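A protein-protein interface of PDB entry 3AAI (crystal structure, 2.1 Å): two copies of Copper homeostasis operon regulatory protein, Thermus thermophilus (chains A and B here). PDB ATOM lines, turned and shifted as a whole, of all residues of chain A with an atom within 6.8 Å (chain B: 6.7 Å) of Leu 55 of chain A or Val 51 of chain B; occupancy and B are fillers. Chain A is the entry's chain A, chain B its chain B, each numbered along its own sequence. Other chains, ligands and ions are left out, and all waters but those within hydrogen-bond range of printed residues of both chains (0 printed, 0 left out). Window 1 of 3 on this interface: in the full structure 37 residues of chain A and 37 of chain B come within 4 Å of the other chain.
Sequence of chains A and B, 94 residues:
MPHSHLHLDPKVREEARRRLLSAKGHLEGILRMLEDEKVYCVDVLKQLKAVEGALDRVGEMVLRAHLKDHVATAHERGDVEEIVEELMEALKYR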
ATOM      1  N   ARG A  19     -16.714 -12.253  -2.896  1.00  0.00           N
ATOM      2  CA  ARG A  19     -17.021 -12.688  -4.249  1.00  0.00           C
ATOM      3  C   ARG A  19     -16.884 -11.556  -5.256  1.00  0.00           C
ATOM      4  O   ARG A  19     -16.428 -11.762  -6.381  1.00  0.00           O
ATOM      5  CB  ARG A  19     -18.432 -13.274  -4.307  1.00  0.00           C
ATOM      6  CG  ARG A  19     -18.696 -14.307  -3.221  1.00  0.00           C
ATOM      7  CD  ARG A  19     -19.873 -15.197  -3.568  1.00  0.00           C
ATOM      8  NE  ARG A  19     -19.562 -16.020  -4.729  1.00  0.00           N
ATOM      9  CZ  ARG A  19     -20.347 -16.979  -5.205  1.00  0.00           C
ATOM     10  NH1 ARG A  19     -21.507 -17.247  -4.619  1.00  0.00           N
ATOM     11  NH2 ARG A  19     -19.964 -17.672  -6.271  1.00  0.00           N
ATOM     12  N   LEU A  20     -17.252 -10.347  -4.851  1.00  0.00           N
ATOM     13  CA  LEU A  20     -17.168  -9.227  -5.765  1.00  0.00           C
ATOM     14  C   LEU A  20     -15.745  -8.727  -5.936  1.00  0.00           C
ATOM     15  O   LEU A  20     -15.415  -8.115  -6.949  1.00  0.00           O
ATOM     16  CB  LEU A  20     -18.092  -8.103  -5.298  1.00  0.00           C
ATOM     17  CG  LEU A  20     -19.580  -8.449  -5.407  1.00  0.00           C
ATOM     18  CD1 LEU A  20     -20.401  -7.286  -4.890  1.00  0.00           C
ATOM     19  CD2 LEU A  20     -19.933  -8.753  -6.862  1.00  0.00           C
ATOM     20  N   ALA A  23     -14.469 -10.915  -8.579  1.00  0.00           N
ATOM     21  CA  ALA A  23     -15.114 -10.512  -9.823  1.00  0.00           C
ATOM     22  C   ALA A  23     -14.389  -9.285 -10.372  1.00  0.00           C
ATOM     23  O   ALA A  23     -14.096  -9.208 -11.566  1.00  0.00           O
ATOM     24  CB  ALA A  23     -16.586 -10.198  -9.573  1.00  0.00           C
ATOM     25  N   LYS A  24     -14.096  -8.328  -9.495  1.00  0.00           N
ATOM     26  CA  LYS A  24     -13.389  -7.113  -9.905  1.00  0.00           C
ATOM     27  C   LYS A  24     -11.989  -7.466 -10.426  1.00  0.00           C
ATOM     28  O   LYS A  24     -11.525  -6.913 -11.424  1.00  0.00           O
ATOM     29  CB  LYS A  24     -13.281  -6.139  -8.729  1.00  0.00           C
ATOM     30  CG  LYS A  24     -12.265  -5.031  -8.939  1.00  0.00           C
ATOM     31  CD  LYS A  24     -12.027  -4.259  -7.661  1.00  0.00           C
ATOM     32  CE  LYS A  24     -10.694  -3.539  -7.697  1.00  0.00           C
ATOM     33  NZ  LYS A  24      -9.556  -4.496  -7.742  1.00  0.00           N
ATOM     34  N   LEU A  27     -12.431  -8.733 -13.762  1.00  0.00           N
ATOM     35  CA  LEU A  27     -12.753  -7.630 -14.657  1.00  0.00           C
ATOM     36  C   LEU A  27     -11.491  -6.916 -15.139  1.00  0.00           C
ATOM     37  O   LEU A  27     -11.394  -6.535 -16.309  1.00  0.00           O
ATOM     38  CB  LEU A  27     -13.693  -6.643 -13.950  1.00  0.00           C
ATOM     39  CG  LEU A  27     -14.542  -5.720 -14.826  1.00  0.00           C
ATOM     40  CD1 LEU A  27     -15.211  -6.534 -15.934  1.00  0.00           C
ATOM     41  CD2 LEU A  27     -15.604  -5.024 -13.955  1.00  0.00           C
ATOM     42  N   LEU A  48     -16.134 -12.166 -20.337  1.00  0.00           N
ATOM     43  CA  LEU A  48     -17.229 -11.278 -19.959  1.00  0.00           C
ATOM     44  C   LEU A  48     -18.411 -12.063 -19.408  1.00  0.00           C
ATOM     45  O   LEU A  48     -18.992 -11.697 -18.381  1.00  0.00           O
ATOM     46  CB  LEU A  48     -17.687 -10.450 -21.162  1.00  0.00           C
ATOM     47  CG  LEU A  48     -16.775  -9.299 -21.566  1.00  0.00           C
ATOM     48  CD1 LEU A  48     -17.228  -8.745 -22.909  1.00  0.00           C
ATOM     49  CD2 LEU A  48     -16.789  -8.223 -20.478  1.00  0.00           C
ATOM     50  N   ALA A  50     -18.280 -14.920 -18.109  1.00  0.00           N
ATOM     51  CA  ALA A  50     -17.835 -15.538 -16.867  1.00  0.00           C
ATOM     52  C   ALA A  50     -18.003 -14.531 -15.726  1.00  0.00           C
ATOM     53  O   ALA A  50     -18.495 -14.875 -14.652  1.00  0.00           O
ATOM     54  CB  ALA A  50     -16.355 -15.980 -16.992  1.00  0.00           C
ATOM     55  N   VAL A  51     -17.589 -13.291 -15.959  1.00  0.00           N
ATOM     56  CA  VAL A  51     -17.728 -12.249 -14.951  1.00  0.00           C
ATOM     57  C   VAL A  51     -19.211 -11.999 -14.690  1.00  0.00           C
ATOM     58  O   VAL A  51     -19.625 -11.822 -13.541  1.00  0.00           O
ATOM     59  CB  VAL A  51     -17.048 -10.936 -15.397  1.00  0.00           C
ATOM     60  CG1 VAL A  51     -17.365  -9.807 -14.412  1.00  0.00           C
ATOM     61  CG2 VAL A  51     -15.536 -11.145 -15.463  1.00  0.00           C
ATOM     62  N   GLU A  52     -20.010 -11.999 -15.753  1.00  0.00           N
ATOM     63  CA  GLU A  52     -21.446 -11.786 -15.604  1.00  0.00           C
ATOM     64  C   GLU A  52     -22.033 -12.893 -14.737  1.00  0.00           C
ATOM     65  O   GLU A  52     -22.931 -12.649 -13.932  1.00  0.00           O
ATOM     66  CB  GLU A  52     -22.142 -11.775 -16.971  1.00  0.00           C
ATOM     67  CG  GLU A  52     -21.635 -10.683 -17.899  1.00  0.00           C
ATOM     68  CD  GLU A  52     -22.437 -10.567 -19.182  1.00  0.00           C
ATOM     69  OE1 GLU A  52     -22.653 -11.597 -19.857  1.00  0.00           O
ATOM     70  OE2 GLU A  52     -22.843  -9.437 -19.520  1.00  0.00           O
ATOM     71  N   GLY A  53     -21.508 -14.108 -14.895  1.00  0.00           N
ATOM     72  CA  GLY A  53     -21.985 -15.232 -14.103  1.00  0.00           C
ATOM     73  C   GLY A  53     -21.651 -15.084 -12.625  1.00  0.00           C
ATOM     74  O   GLY A  53     -22.461 -15.414 -11.757  1.00  0.00           O
ATOM     75  N   ALA A  54     -20.453 -14.590 -12.327  1.00  0.00           N
ATOM     76  CA  ALA A  54     -20.049 -14.405 -10.942  1.00  0.00           C
ATOM     77  C   ALA A  54     -20.934 -13.341 -10.276  1.00  0.00           C
ATOM     78  O   ALA A  54     -21.289 -13.460  -9.105  1.00  0.00           O
ATOM     79  CB  ALA A  54     -18.576 -13.999 -10.876  1.00  0.00           C
ATOM     80  N   LEU A  55     -21.283 -12.303 -11.030  1.00  0.00           N
ATOM     81  CA  LEU A  55     -22.130 -11.231 -10.516  1.00  0.00           C
ATOM     82  C   LEU A  55     -23.515 -11.796 -10.229  1.00  0.00           C
ATOM     83  O   LEU A  55     -24.102 -11.518  -9.182  1.00  0.00           O
ATOM     84  CB  LEU A  55     -22.219 -10.085 -11.533  1.00  0.00           C
ATOM     85  CG  LEU A  55     -20.894  -9.382 -11.857  1.00  0.00           C
ATOM     86  CD1 LEU A  55     -21.127  -8.333 -12.931  1.00  0.00           C
ATOM     87  CD2 LEU A  55     -20.312  -8.739 -10.604  1.00  0.00           C
ATOM     88  N   ASP A  56     -24.021 -12.603 -11.157  1.00  0.00           N
ATOM     89  CA  ASP A  56     -25.324 -13.251 -11.017  1.00  0.00           C
ATOM     90  C   ASP A  56     -25.390 -14.101  -9.749  1.00  0.00           C
ATOM     91  O   ASP A  56     -26.394 -14.080  -9.035  1.00  0.00           O
ATOM     92  CB  ASP A  56     -25.599 -14.147 -12.223  1.00  0.00           C
ATOM     93  CG  ASP A  56     -26.239 -13.401 -13.371  1.00  0.00           C
ATOM     94  OD1 ASP A  56     -26.202 -13.918 -14.509  1.00  0.00           O
ATOM     95  OD2 ASP A  56     -26.790 -12.305 -13.135  1.00  0.00           O
ATOM     96  N   ARG A  57     -24.328 -14.857  -9.475  1.00  0.00           N
ATOM     97  CA  ARG A  57     -24.291 -15.700  -8.281  1.00  0.00           C
ATOM     98  C   ARG A  57     -24.348 -14.873  -6.996  1.00  0.00           C
ATOM     99  O   ARG A  57     -24.911 -15.311  -5.990  1.00  0.00           O
ATOM    100  CB  ARG A  57     -23.040 -16.589  -8.282  1.00  0.00           C
ATOM    101  CG  ARG A  57     -23.093 -17.695  -9.333  1.00  0.00           C
ATOM    102  CD  ARG A  57     -22.014 -18.746  -9.107  1.00  0.00           C
ATOM    103  NE  ARG A  57     -20.675 -18.267  -9.446  1.00  0.00           N
ATOM    104  CZ  ARG A  57     -20.242 -18.069 -10.688  1.00  0.00           C
ATOM    105  NH1 ARG A  57     -19.005 -17.632 -10.895  1.00  0.00           N
ATOM    106  NH2 ARG A  57     -21.038 -18.311 -11.721  1.00  0.00           N
ATOM    107  N   VAL A  58     -23.755 -13.685  -7.021  1.00  0.00           N
ATOM    108  CA  VAL A  58     -23.799 -12.825  -5.849  1.00  0.00           C
ATOM    109  C   VAL A  58     -25.223 -12.272  -5.715  1.00  0.00           C
ATOM    110  O   VAL A  58     -25.784 -12.241  -4.624  1.00  0.00           O
ATOM    111  CB  VAL A  58     -22.801 -11.659  -5.965  1.00  0.00           C
ATOM    112  CG1 VAL A  58     -22.993 -10.690  -4.791  1.00  0.00           C
ATOM    113  CG2 VAL A  58     -21.370 -12.203  -5.957  1.00  0.00           C
ATOM    114  N   GLY A  59     -25.801 -11.836  -6.829  1.00  0.00           N
ATOM    115  CA  GLY A  59     -27.155 -11.311  -6.792  1.00  0.00           C
ATOM    116  C   GLY A  59     -28.099 -12.392  -6.295  1.00  0.00           C
ATOM    117  O   GLY A  59     -29.054 -12.119  -5.565  1.00  0.00           O
ATOM    118  N   GLU A  60     -27.820 -13.630  -6.693  1.00  0.00           N
ATOM    119  CA  GLU A  60     -28.627 -14.775  -6.294  1.00  0.00           C
ATOM    120  C   GLU A  60     -28.578 -14.964  -4.786  1.00  0.00           C
ATOM    121  O   GLU A  60     -29.602 -15.179  -4.140  1.00  0.00           O
ATOM    122  CB  GLU A  60     -28.108 -16.039  -6.975  1.00  0.00           C
ATOM    123  CG  GLU A  60     -29.013 -17.244  -6.813  1.00  0.00           C
ATOM    124  CD  GLU A  60     -28.470 -18.482  -7.500  1.00  0.00           C
ATOM    125  OE1 GLU A  60     -27.917 -18.345  -8.610  1.00  0.00           O
ATOM    126  OE2 GLU A  60     -28.609 -19.587  -6.934  1.00  0.00           O
ATOM    127  N   SER B  22     -15.148   2.100 -16.251  1.00  0.00           N
ATOM    128  CA  SER B  22     -16.274   2.643 -15.517  1.00  0.00           C
ATOM    129  C   SER B  22     -16.991   1.514 -14.782  1.00  0.00           C
ATOM    130  O   SER B  22     -17.427   1.684 -13.641  1.00  0.00           O
ATOM    131  CB  SER B  22     -17.231   3.357 -16.477  1.00  0.00           C
ATOM    132  OG  SER B  22     -17.594   2.515 -17.552  1.00  0.00           O
ATOM    133  N   ALA B  23     -17.105   0.362 -15.439  1.00  0.00           N
ATOM    134  CA  ALA B  23     -17.748  -0.801 -14.850  1.00  0.00           C
ATOM    135  C   ALA B  23     -16.971  -1.194 -13.598  1.00  0.00           C
ATOM    136  O   ALA B  23     -17.552  -1.453 -12.551  1.00  0.00           O
ATOM    137  CB  ALA B  23     -17.762  -1.956 -15.847  1.00  0.00           C
ATOM    138  N   LYS B  24     -15.648  -1.225 -13.719  1.00  0.00           N
ATOM    139  CA  LYS B  24     -14.785  -1.570 -12.598  1.00  0.00           C
ATOM    140  C   LYS B  24     -14.941  -0.524 -11.495  1.00  0.00           C
ATOM    141  O   LYS B  24     -14.989  -0.860 -10.311  1.00  0.00           O
ATOM    142  CB  LYS B  24     -13.324  -1.625 -13.052  1.00  0.00           C
ATOM    143  CG  LYS B  24     -12.354  -2.138 -11.988  1.00  0.00           C
ATOM    144  CD  LYS B  24     -10.957  -2.327 -12.555  1.00  0.00           C
ATOM    145  CE  LYS B  24     -10.171  -1.025 -12.619  1.00  0.00           C
ATOM    146  NZ  LYS B  24      -9.761  -0.546 -11.264  1.00  0.00           N
ATOM    147  N   HIS B  26     -17.516   1.248 -10.889  1.00  0.00           N
ATOM    148  CA  HIS B  26     -18.825   1.021 -10.298  1.00  0.00           C
ATOM    149  C   HIS B  26     -18.804  -0.202  -9.362  1.00  0.00           C
ATOM    150  O   HIS B  26     -19.470  -0.221  -8.331  1.00  0.00           O
ATOM    151  CB  HIS B  26     -19.858   0.808 -11.409  1.00  0.00           C
ATOM    152  CG  HIS B  26     -21.273   0.995 -10.966  1.00  0.00           C
ATOM    153  ND1 HIS B  26     -22.344   0.468 -11.653  1.00  0.00           N
ATOM    154  CD2 HIS B  26     -21.797   1.679  -9.921  1.00  0.00           C
ATOM    155  CE1 HIS B  26     -23.467   0.817 -11.051  1.00  0.00           C
ATOM    156  NE2 HIS B  26     -23.162   1.552  -9.997  1.00  0.00           N
ATOM    157  N   LEU B  27     -18.032  -1.223  -9.715  1.00  0.00           N
ATOM    158  CA  LEU B  27     -17.971  -2.418  -8.875  1.00  0.00           C
ATOM    159  C   LEU B  27     -17.225  -2.119  -7.575  1.00  0.00           C
ATOM    160  O   LEU B  27     -17.563  -2.649  -6.514  1.00  0.00           O
ATOM    161  CB  LEU B  27     -17.293  -3.564  -9.635  1.00  0.00           C
ATOM    162  CG  LEU B  27     -17.299  -4.968  -9.021  1.00  0.00           C
ATOM    163  CD1 LEU B  27     -18.713  -5.376  -8.626  1.00  0.00           C
ATOM    164  CD2 LEU B  27     -16.722  -5.953 -10.031  1.00  0.00           C
ATOM    165  N   ILE B  30     -19.603  -0.568  -5.199  1.00  0.00           N
ATOM    166  CA  ILE B  30     -20.483  -1.527  -4.540  1.00  0.00           C
ATOM    167  C   ILE B  30     -19.715  -2.166  -3.380  1.00  0.00           C
ATOM    168  O   ILE B  30     -20.254  -2.328  -2.277  1.00  0.00           O
ATOM    169  CB  ILE B  30     -20.947  -2.646  -5.516  1.00  0.00           C
ATOM    170  CG1 ILE B  30     -21.690  -2.035  -6.706  1.00  0.00           C
ATOM    171  CG2 ILE B  30     -21.836  -3.640  -4.790  1.00  0.00           C
ATOM    172  CD1 ILE B  30     -22.239  -3.068  -7.677  1.00  0.00           C
ATOM    173  N   LYS B  46     -29.709  -3.814  -7.622  1.00  0.00           N
ATOM    174  CA  LYS B  46     -29.845  -2.823  -8.679  1.00  0.00           C
ATOM    175  C   LYS B  46     -28.500  -2.425  -9.270  1.00  0.00           C
ATOM    176  O   LYS B  46     -28.338  -2.339 -10.490  1.00  0.00           O
ATOM    177  CB  LYS B  46     -30.542  -1.564  -8.149  1.00  0.00           C
ATOM    178  CG  LYS B  46     -32.031  -1.707  -7.910  1.00  0.00           C
ATOM    179  CD  LYS B  46     -32.628  -0.365  -7.518  1.00  0.00           C
ATOM    180  CE  LYS B  46     -34.140  -0.433  -7.426  1.00  0.00           C
ATOM    181  NZ  LYS B  46     -34.726   0.911  -7.154  1.00  0.00           N
ATOM    182  N   GLN B  47     -27.541  -2.153  -8.398  1.00  0.00           N
ATOM    183  CA  GLN B  47     -26.219  -1.747  -8.853  1.00  0.00           C
ATOM    184  C   GLN B  47     -25.503  -2.890  -9.563  1.00  0.00           C
ATOM    185  O   GLN B  47     -24.749  -2.661 -10.503  1.00  0.00           O
ATOM    186  CB  GLN B  47     -25.396  -1.241  -7.670  1.00  0.00           C
ATOM    187  CG  GLN B  47     -25.967   0.027  -7.039  1.00  0.00           C
ATOM    188  CD  GLN B  47     -26.342   1.074  -8.075  1.00  0.00           C
ATOM    189  OE1 GLN B  47     -25.559   1.383  -8.975  1.00  0.00           O
ATOM    190  NE2 GLN B  47     -27.543   1.628  -7.951  1.00  0.00           N
ATOM    191  N   LEU B  48     -25.736  -4.118  -9.116  1.00  0.00           N
ATOM    192  CA  LEU B  48     -25.110  -5.258  -9.772  1.00  0.00           C
ATOM    193  C   LEU B  48     -25.678  -5.336 -11.185  1.00  0.00           C
ATOM    194  O   LEU B  48     -24.948  -5.582 -12.145  1.00  0.00           O
ATOM    195  CB  LEU B  48     -25.397  -6.549  -9.001  1.00  0.00           C
ATOM    196  CG  LEU B  48     -24.589  -6.684  -7.705  1.00  0.00           C
ATOM    197  CD1 LEU B  48     -25.082  -7.872  -6.884  1.00  0.00           C
ATOM    198  CD2 LEU B  48     -23.116  -6.834  -8.051  1.00  0.00           C
ATOM    199  N   LYS B  49     -26.984  -5.112 -11.305  1.00  0.00           N
ATOM    200  CA  LYS B  49     -27.636  -5.142 -12.608  1.00  0.00           C
ATOM    201  C   LYS B  49     -27.026  -4.090 -13.521  1.00  0.00           C
ATOM    202  O   LYS B  49     -26.927  -4.291 -14.730  1.00  0.00           O
ATOM    203  CB  LYS B  49     -29.141  -4.886 -12.468  1.00  0.00           C
ATOM    204  CG  LYS B  49     -29.921  -6.021 -11.828  1.00  0.00           C
ATOM    205  CD  LYS B  49     -29.818  -7.296 -12.653  1.00  0.00           C
ATOM    206  CE  LYS B  49     -30.505  -8.461 -11.960  1.00  0.00           C
ATOM    207  NZ  LYS B  49     -30.198  -9.751 -12.638  1.00  0.00           N
ATOM    208  N   ALA B  50     -26.603  -2.969 -12.938  1.00  0.00           N
ATOM    209  CA  ALA B  50     -26.000  -1.885 -13.710  1.00  0.00           C
ATOM    210  C   ALA B  50     -24.626  -2.294 -14.234  1.00  0.00           C
ATOM    211  O   ALA B  50     -24.270  -2.002 -15.376  1.00  0.00           O
ATOM    212  CB  ALA B  50     -25.885  -0.634 -12.854  1.00  0.00           C
ATOM    213  N   VAL B  51     -23.846  -2.963 -13.396  1.00  0.00           N
ATOM    214  CA  VAL B  51     -22.528  -3.417 -13.823  1.00  0.00           C
ATOM    215  C   VAL B  51     -22.718  -4.409 -14.976  1.00  0.00           C
ATOM    216  O   VAL B  51     -22.002  -4.368 -15.975  1.00  0.00           O
ATOM    217  CB  VAL B  51     -21.767  -4.108 -12.655  1.00  0.00           C
ATOM    218  CG1 VAL B  51     -20.480  -4.760 -13.157  1.00  0.00           C
ATOM    219  CG2 VAL B  51     -21.445  -3.082 -11.574  1.00  0.00           C
ATOM    220  N   GLU B  52     -23.704  -5.286 -14.837  1.00  0.00           N
ATOM    221  CA  GLU B  52     -23.971  -6.284 -15.864  1.00  0.00           C
ATOM    222  C   GLU B  52     -24.368  -5.610 -17.171  1.00  0.00           C
ATOM    223  O   GLU B  52     -23.935  -6.015 -18.248  1.00  0.00           O
ATOM    224  CB  GLU B  52     -25.079  -7.235 -15.398  1.00  0.00           C
ATOM    225  CG  GLU B  52     -24.722  -8.008 -14.137  1.00  0.00           C
ATOM    226  CD  GLU B  52     -25.771  -9.033 -13.751  1.00  0.00           C
ATOM    227  OE1 GLU B  52     -26.922  -8.637 -13.465  1.00  0.00           O
ATOM    228  OE2 GLU B  52     -25.441 -10.238 -13.732  1.00  0.00           O
ATOM    229  N   GLY B  53     -25.186  -4.568 -17.067  1.00  0.00           N
ATOM    230  CA  GLY B  53     -25.616  -3.854 -18.251  1.00  0.00           C
ATOM    231  C   GLY B  53     -24.452  -3.263 -19.014  1.00  0.00           C
ATOM    232  O   GLY B  53     -24.455  -3.250 -20.243  1.00  0.00           O
ATOM    233  N   ALA B  54     -23.452  -2.772 -18.290  1.00  0.00           N
ATOM    234  CA  ALA B  54     -22.274  -2.187 -18.921  1.00  0.00           C
ATOM    235  C   ALA B  54     -21.406  -3.268 -19.579  1.00  0.00           C
ATOM    236  O   ALA B  54     -20.790  -3.028 -20.619  1.00  0.00           O
ATOM    237  CB  ALA B  54     -21.457  -1.411 -17.887  1.00  0.00           C
ATOM    238  N   LEU B  55     -21.355  -4.451 -18.969  1.00  0.00           N
ATOM    239  CA  LEU B  55     -20.567  -5.553 -19.523  1.00  0.00           C
ATOM    240  C   LEU B  55     -21.214  -6.016 -20.828  1.00  0.00           C
ATOM    241  O   LEU B  55     -20.524  -6.369 -21.786  1.00  0.00           O
ATOM    242  CB  LEU B  55     -20.489  -6.719 -18.527  1.00  0.00           C
ATOM    243  CG  LEU B  55     -19.802  -6.461 -17.179  1.00  0.00           C
ATOM    244  CD1 LEU B  55     -19.764  -7.746 -16.370  1.00  0.00           C
ATOM    245  CD2 LEU B  55     -18.390  -5.949 -17.397  1.00  0.00           C
ATOM    246  N   ASP B  56     -22.544  -6.007 -20.860  1.00  0.00           N
ATOM    247  CA  ASP B  56     -23.281  -6.399 -22.057  1.00  0.00           C
ATOM    248  C   ASP B  56     -22.933  -5.481 -23.227  1.00  0.00           C
ATOM    249  O   ASP B  56     -22.791  -5.936 -24.360  1.00  0.00           O
ATOM    250  CB  ASP B  56     -24.790  -6.345 -21.792  1.00  0.00           C
ATOM    251  CG  ASP B  56     -25.296  -7.569 -21.054  1.00  0.00           C
ATOM    252  OD1 ASP B  56     -26.414  -7.510 -20.494  1.00  0.00           O
ATOM    253  OD2 ASP B  56     -24.584  -8.595 -21.046  1.00  0.00           O
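Leu 27 of chain A touches Leu 55 of chain B, but with the chains exchanged Leu 55 of chain A does not touch Leu 27 of chain B (4.2 Å). Val 51 of chain A touches Leu 55 of chain B, and with the chains exchanged Leu 55 of chain A touches Val 51 of chain B. Glu 52 of chain B touches its own counterpart, Glu 52 of chain A. Glu 52 of chain A touches Asp 56 of chain B, and with the chains exchanged Asp 56 of chain A touches Glu 52 of chain B. 11 positions are printed for both chains. Of the 14 pairs that touch across the chains among the printed residues, 10 have their exchanged pair printed and touching as well.
The side-chain amino group of Lys 49 of chain B lies within salt-bridge range of the side-chain carboxylate of Glu 52 of chain B, 3.6 Å away.
Of chain B, only Val 51, Glu 52 and Leu 55 come within 4 Å of Leu 55 of chain A. Val 51 of chain B touches one residue of chain A. Printed residues of chain A within 4 Å of Lys 24 of chain B: Leu 27 (3.8 Å). Of the printed residues of chain B, Asp 56 of chain A touches Glu 52 (2.5 Å). Printed residues of chain A within 4 Å of Asp 56 of chain B: Glu 52. Glu 60 of chain A touches none of the printed residues of chain B. The nearest residue of chain A that does not touch Val 51 of chain B is Leu 27 of chain A (4.9 Å). The nearest printed residue of chain A that does not touch Leu 55 of chain B is Leu 48 of chain A (4.2 Å).
Among the printed residues, merely in contact across the chains: Lys 24 of chain A with Leu 27 of chain B, Leu 27 of chain A with Leu 55 of chain B, Leu 55 of chain A with Val 51 of chain B, Val 51 of chain A with Leu 55 of chain B, Glu 52 of chain A with Leu 55 of chain B, Leu 55 of chain A with Leu 55 of chain B, Leu 27 of chain A with Lys 24 of chain B, Leu 55 of chain A with Glu 52 of chain B, Leu 20 of chain A with Leu 48 of chain B, Leu 20 of chain A with Ile 30 of chain B and Leu 20 of chain A with Leu 27 of chain B.
The side-chain carboxylate (OE2) of Glu 52 of chain A sits close to the side-chain carboxylate (OD2) of Asp 56 of chain B (2.5 Å). OE2 of Glu 52 of chain B lies close to OD2 of Asp 56 of chain A (2.5 Å). The backbone carbonyl oxygen of Glu 52 of chain A sits close to the side-chain carboxylate of Glu 52 of chain B (3.5 Å).
Of the 17 printed residues of chain B, 8 touch a printed residue of chain A. Hydrophobic or aromatic side chains of chain B within 4 Å of the printed part of chain A: Leu 27, Ile 30, Leu 48, Val 51 and Leu 55. Of the 17 printed residues of chain A, 7 touch a printed residue of chain B. Printed residues of chain A that touch a printed residue of chain B: Leu 20, Lys 24, Leu 27, Val 51, Glu 52, Leu 55 and Asp 56. Hydrophobic or aromatic side chains of chain A within 4 Å of the printed part of chain B: Leu 20, Leu 27, Val 51 and Leu 55. Among the printed residues, 14 pairs touch across the chains. Among the printed residues, no Asp or Glu carboxylate lies within 4 Å of a Lys or Arg side-chain nitrogen of the other chain.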
